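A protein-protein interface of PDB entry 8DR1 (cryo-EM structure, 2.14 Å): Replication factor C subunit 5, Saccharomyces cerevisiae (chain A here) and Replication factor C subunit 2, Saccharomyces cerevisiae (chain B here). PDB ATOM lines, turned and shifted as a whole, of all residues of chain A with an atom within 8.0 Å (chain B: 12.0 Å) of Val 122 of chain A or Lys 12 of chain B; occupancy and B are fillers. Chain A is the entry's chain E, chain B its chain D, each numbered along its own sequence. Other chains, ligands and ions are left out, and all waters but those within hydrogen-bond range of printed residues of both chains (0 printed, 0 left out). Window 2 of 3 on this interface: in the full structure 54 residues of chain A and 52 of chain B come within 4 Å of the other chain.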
ATOM      1  N   MET A 119     -12.925  10.702 -30.072  1.00  0.00           N
ATOM      2  CA  MET A 119     -12.145   9.581 -29.563  1.00  0.00           C
ATOM      3  C   MET A 119     -13.023   8.713 -28.676  1.00  0.00           C
ATOM      4  O   MET A 119     -13.673   9.217 -27.756  1.00  0.00           O
ATOM      5  CB  MET A 119     -10.926  10.071 -28.775  1.00  0.00           C
ATOM      6  CG  MET A 119      -9.595   9.762 -29.443  1.00  0.00           C
ATOM      7  SD  MET A 119      -8.172  10.388 -28.527  1.00  0.00           S
ATOM      8  CE  MET A 119      -8.546  12.138 -28.450  1.00  0.00           C
ATOM      9  N   GLU A 120     -13.035   7.414 -28.954  1.00  0.00           N
ATOM     10  CA  GLU A 120     -13.756   6.456 -28.132  1.00  0.00           C
ATOM     11  C   GLU A 120     -12.859   5.947 -27.008  1.00  0.00           C
ATOM     12  O   GLU A 120     -11.629   5.948 -27.112  1.00  0.00           O
ATOM     13  CB  GLU A 120     -14.257   5.286 -28.980  1.00  0.00           C
ATOM     14  CG  GLU A 120     -15.172   5.701 -30.121  1.00  0.00           C
ATOM     15  CD  GLU A 120     -15.695   4.516 -30.909  1.00  0.00           C
ATOM     16  OE1 GLU A 120     -15.399   3.366 -30.522  1.00  0.00           O
ATOM     17  OE2 GLU A 120     -16.402   4.735 -31.915  1.00  0.00           O
ATOM     18  N   GLN A 121     -13.493   5.508 -25.926  1.00  0.00           N
ATOM     19  CA  GLN A 121     -12.777   5.056 -24.740  1.00  0.00           C
ATOM     20  C   GLN A 121     -12.463   3.572 -24.872  1.00  0.00           C
ATOM     21  O   GLN A 121     -13.376   2.742 -24.951  1.00  0.00           O
ATOM     22  CB  GLN A 121     -13.601   5.320 -23.481  1.00  0.00           C
ATOM     23  CG  GLN A 121     -12.936   4.836 -22.201  1.00  0.00           C
ATOM     24  CD  GLN A 121     -13.417   5.579 -20.969  1.00  0.00           C
ATOM     25  OE1 GLN A 121     -14.140   6.571 -21.068  1.00  0.00           O
ATOM     26  NE2 GLN A 121     -13.017   5.099 -19.797  1.00  0.00           N
ATOM     27  N   VAL A 122     -11.172   3.241 -24.894  1.00  0.00           N
ATOM     28  CA  VAL A 122     -10.721   1.856 -24.969  1.00  0.00           C
ATOM     29  C   VAL A 122     -10.017   1.399 -23.702  1.00  0.00           C
ATOM     30  O   VAL A 122      -9.817   0.185 -23.528  1.00  0.00           O
ATOM     31  CB  VAL A 122      -9.803   1.627 -26.190  1.00  0.00           C
ATOM     32  CG1 VAL A 122     -10.316   2.404 -27.393  1.00  0.00           C
ATOM     33  CG2 VAL A 122      -8.368   2.024 -25.867  1.00  0.00           C
ATOM     34  N   ASP A 123      -9.636   2.316 -22.815  1.00  0.00           N
ATOM     35  CA  ASP A 123      -9.009   1.930 -21.559  1.00  0.00           C
ATOM     36  C   ASP A 123     -10.047   1.328 -20.622  1.00  0.00           C
ATOM     37  O   ASP A 123     -11.135   1.886 -20.441  1.00  0.00           O
ATOM     38  CB  ASP A 123      -8.343   3.140 -20.906  1.00  0.00           C
ATOM     39  CG  ASP A 123      -7.263   3.750 -21.777  1.00  0.00           C
ATOM     40  OD1 ASP A 123      -7.077   3.274 -22.917  1.00  0.00           O
ATOM     41  OD2 ASP A 123      -6.600   4.706 -21.323  1.00  0.00           O
ATOM     42  N   PHE A 124      -9.708   0.190 -20.014  1.00  0.00           N
ATOM     43  CA  PHE A 124     -10.635  -0.540 -19.150  1.00  0.00           C
ATOM     44  C   PHE A 124     -10.754   0.196 -17.818  1.00  0.00           C
ATOM     45  O   PHE A 124     -10.095  -0.122 -16.826  1.00  0.00           O
ATOM     46  CB  PHE A 124     -10.166  -1.976 -18.951  1.00  0.00           C
ATOM     47  CG  PHE A 124     -11.129  -2.824 -18.170  1.00  0.00           C
ATOM     48  CD1 PHE A 124     -12.387  -3.109 -18.674  1.00  0.00           C
ATOM     49  CD2 PHE A 124     -10.777  -3.335 -16.932  1.00  0.00           C
ATOM     50  CE1 PHE A 124     -13.276  -3.888 -17.958  1.00  0.00           C
ATOM     51  CE2 PHE A 124     -11.662  -4.114 -16.211  1.00  0.00           C
ATOM     52  CZ  PHE A 124     -12.913  -4.391 -16.725  1.00  0.00           C
ATOM     53  N   GLN A 125     -11.623   1.210 -17.803  1.00  0.00           N
ATOM     54  CA  GLN A 125     -11.901   1.985 -16.594  1.00  0.00           C
ATOM     55  C   GLN A 125     -13.137   1.393 -15.923  1.00  0.00           C
ATOM     56  O   GLN A 125     -14.246   1.926 -15.997  1.00  0.00           O
ATOM     57  CB  GLN A 125     -12.090   3.457 -16.933  1.00  0.00           C
ATOM     58  CG  GLN A 125     -10.835   4.141 -17.449  1.00  0.00           C
ATOM     59  CD  GLN A 125     -10.976   5.650 -17.503  1.00  0.00           C
ATOM     60  OE1 GLN A 125     -12.080   6.178 -17.630  1.00  0.00           O
ATOM     61  NE2 GLN A 125      -9.854   6.352 -17.406  1.00  0.00           N
ATOM     62  N   ALA A 132     -16.729  -0.987 -18.015  1.00  0.00           N
ATOM     63  CA  ALA A 132     -15.815   0.136 -18.145  1.00  0.00           C
ATOM     64  C   ALA A 132     -16.560   1.400 -18.560  1.00  0.00           C
ATOM     65  O   ALA A 132     -17.561   1.352 -19.282  1.00  0.00           O
ATOM     66  CB  ALA A 132     -14.723  -0.177 -19.167  1.00  0.00           C
ATOM     67  N   HIS A 133     -16.059   2.541 -18.092  1.00  0.00           N
ATOM     68  CA  HIS A 133     -16.624   3.822 -18.493  1.00  0.00           C
ATOM     69  C   HIS A 133     -16.476   4.010 -19.997  1.00  0.00           C
ATOM     70  O   HIS A 133     -15.483   3.591 -20.597  1.00  0.00           O
ATOM     71  CB  HIS A 133     -15.932   4.965 -17.750  1.00  0.00           C
ATOM     72  CG  HIS A 133     -16.068   4.887 -16.261  1.00  0.00           C
ATOM     73  ND1 HIS A 133     -15.002   4.617 -15.430  1.00  0.00           N
ATOM     74  CD2 HIS A 133     -17.143   5.045 -15.453  1.00  0.00           C
ATOM     75  CE1 HIS A 133     -15.415   4.611 -14.175  1.00  0.00           C
ATOM     76  NE2 HIS A 133     -16.710   4.868 -14.162  1.00  0.00           N
ATOM     77  N   ARG A 134     -17.477   4.642 -20.608  1.00  0.00           N
ATOM     78  CA  ARG A 134     -17.499   4.839 -22.049  1.00  0.00           C
ATOM     79  C   ARG A 134     -17.286   6.286 -22.470  1.00  0.00           C
ATOM     80  O   ARG A 134     -17.080   6.537 -23.663  1.00  0.00           O
ATOM     81  CB  ARG A 134     -18.831   4.339 -22.628  1.00  0.00           C
ATOM     82  CG  ARG A 134     -19.015   2.834 -22.529  1.00  0.00           C
ATOM     83  CD  ARG A 134     -18.147   2.099 -23.538  1.00  0.00           C
ATOM     84  NE  ARG A 134     -18.207   0.653 -23.364  1.00  0.00           N
ATOM     85  CZ  ARG A 134     -17.686  -0.227 -24.208  1.00  0.00           C
ATOM     86  NH1 ARG A 134     -17.061   0.159 -25.310  1.00  0.00           N
ATOM     87  NH2 ARG A 134     -17.796  -1.525 -23.943  1.00  0.00           N
ATOM     88  N   ARG B  11      -4.912  -0.923 -22.106  1.00  0.00           N
ATOM     89  CA  ARG B  11      -5.752  -2.057 -22.471  1.00  0.00           C
ATOM     90  C   ARG B  11      -6.731  -1.672 -23.575  1.00  0.00           C
ATOM     91  O   ARG B  11      -6.650  -0.579 -24.135  1.00  0.00           O
ATOM     92  CB  ARG B  11      -6.514  -2.575 -21.249  1.00  0.00           C
ATOM     93  N   LYS B  12      -7.656  -2.579 -23.882  1.00  0.00           N
ATOM     94  CA  LYS B  12      -8.654  -2.354 -24.917  1.00  0.00           C
ATOM     95  C   LYS B  12     -10.016  -2.804 -24.409  1.00  0.00           C
ATOM     96  O   LYS B  12     -10.116  -3.663 -23.529  1.00  0.00           O
ATOM     97  CB  LYS B  12      -8.303  -3.104 -26.210  1.00  0.00           C
ATOM     98  CG  LYS B  12      -8.822  -2.438 -27.476  1.00  0.00           C
ATOM     99  CD  LYS B  12      -8.000  -1.212 -27.843  1.00  0.00           C
ATOM    100  CE  LYS B  12      -8.568  -0.510 -29.067  1.00  0.00           C
ATOM    101  NZ  LYS B  12      -7.665   0.562 -29.568  1.00  0.00           N
ATOM    102  N   ILE B  13     -11.065  -2.212 -24.976  1.00  0.00           N
ATOM    103  CA  ILE B  13     -12.444  -2.535 -24.636  1.00  0.00           C
ATOM    104  C   ILE B  13     -13.159  -2.994 -25.897  1.00  0.00           C
ATOM    105  O   ILE B  13     -13.007  -2.388 -26.964  1.00  0.00           O
ATOM    106  CB  ILE B  13     -13.180  -1.333 -24.007  1.00  0.00           C
ATOM    107  CG1 ILE B  13     -12.675  -1.077 -22.587  1.00  0.00           C
ATOM    108  CG2 ILE B  13     -14.683  -1.579 -23.997  1.00  0.00           C
ATOM    109  CD1 ILE B  13     -12.994   0.312 -22.072  1.00  0.00           C
ATOM    110  N   SER B  14     -13.939  -4.064 -25.773  1.00  0.00           N
ATOM    111  CA  SER B  14     -14.738  -4.534 -26.895  1.00  0.00           C
ATOM    112  C   SER B  14     -15.748  -3.469 -27.302  1.00  0.00           C
ATOM    113  O   SER B  14     -16.405  -2.856 -26.457  1.00  0.00           O
ATOM    114  CB  SER B  14     -15.457  -5.832 -26.527  1.00  0.00           C
ATOM    115  OG  SER B  14     -16.343  -5.632 -25.439  1.00  0.00           O
ATOM    116  N   LYS B  15     -15.869  -3.249 -28.610  1.00  0.00           N
ATOM    117  CA  LYS B  15     -16.771  -2.222 -29.111  1.00  0.00           C
ATOM    118  C   LYS B  15     -18.214  -2.553 -28.745  1.00  0.00           C
ATOM    119  O   LYS B  15     -18.629  -3.714 -28.768  1.00  0.00           O
ATOM    120  CB  LYS B  15     -16.630  -2.091 -30.627  1.00  0.00           C
ATOM    121  CG  LYS B  15     -15.285  -1.542 -31.076  1.00  0.00           C
ATOM    122  CD  LYS B  15     -15.203  -1.440 -32.589  1.00  0.00           C
ATOM    123  CE  LYS B  15     -13.896  -0.806 -33.035  1.00  0.00           C
ATOM    124  NZ  LYS B  15     -13.792  -0.721 -34.518  1.00  0.00           N
ATOM    125  N   LEU B  16     -18.975  -1.519 -28.406  1.00  0.00           N
ATOM    126  CA  LEU B  16     -20.374  -1.675 -28.040  1.00  0.00           C
ATOM    127  C   LEU B  16     -21.259  -1.684 -29.283  1.00  0.00           C
ATOM    128  O   LEU B  16     -20.916  -1.125 -30.328  1.00  0.00           O
ATOM    129  CB  LEU B  16     -20.816  -0.552 -27.101  1.00  0.00           C
ATOM    130  CG  LEU B  16     -20.834  -0.880 -25.608  1.00  0.00           C
ATOM    131  CD1 LEU B  16     -20.948   0.395 -24.792  1.00  0.00           C
ATOM    132  CD2 LEU B  16     -21.971  -1.834 -25.276  1.00  0.00           C
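The backbone carbonyl oxygen of Val 122 of chain A lies within hydrogen-bond range of the backbone NH of Ile 13 of chain B (3.1 Å). NH2 of Arg 134 of chain A is in hydrogen-bond range of O of Ser 14 of chain B (3.2 Å). The backbone carbonyl oxygen of Arg 11 of chain B lies close to the backbone carbonyl oxygen of Val 122 of chain A, 3.3 Å away.
Of the 10 printed residues of chain A, 6 touch a printed residue of chain B. Hydrophobic or aromatic side chains of chain A within 4 Å of the printed part of chain B: Val 122 and Ala 132. Of the 6 printed residues of chain B, 5 touch a printed residue of chain A. Printed residues of chain B that touch a printed residue of chain A: Arg 11, Lys 12, Ile 13, Ser 14 and Leu 16. Hydrophobic or aromatic side chains of chain B that line the printed part of chain A: Ile 13 and Leu 16. Among the printed residues, 10 pairs touch across the chains.
Gln 121 of chain A touches Ile 13 of chain B. Val 122 of chain A touches Lys 12 of chain B (O to CA, 3.1 Å). Asp 123 of chain A touches Ile 13 of chain B. CA of Phe 124 of chain A touches CD1 of Ile 13 of chain B, 3.9 Å away. Ala 132 of chain A touches Ile 13 of chain B. Arg 134 of chain A touches Ile 13 of chain B. Arg 134 of chain A touches Leu 16 of chain B (NE to CD1, 3.1 Å).
No residue of chain B comes within 4 Å of Glu 120 of chain A. Gln 121 of chain A touches one residue of chain B. Val 122 of chain A touches just these residues of chain B: Arg 11, Lys 12 and Ile 13. Asp 123 of chain A touches one residue of chain B. Gln 125 of chain A touches none of the printed residues of chain B. Of the printed residues of chain B, Ala 132 of chain A touches Ile 13. Of the printed residues of chain B, Arg 134 of chain A touches Ile 13, Ser 14 and Leu 16. Arg 11 of chain B touches just one residue of chain A: Val 122 (3.3 Å). Of the printed residues of chain A, Ile 13 of chain B touches Gln 121 (3.8 Å), Val 122 (3.1 Å), Asp 123 (2.9 Å), Phe 124 (3.9 Å), Ala 132 (3.4 Å) and Arg 134 (3.1 Å). Of the printed residues of chain A, Ser 14 of chain B touches Arg 134 (3.2 Å). Of the printed residues of chain A, Leu 16 of chain B touches Arg 134. The nearest residue of chain B that does not touch Val 122 of chain A is Ser 14 of chain B (6.3 Å). The nearest residue of chain A that does not touch Lys 12 of chain B is Phe 124 of chain A (4.9 Å).
The side-chain amide nitrogen of Gln 121 of chain A lies within hydrogen-bond range of the side-chain amide oxygen of Gln 125 of chain A. O of His 133 of chain A sits close to NE2 of Gln 121 of chain A (3.0 Å).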
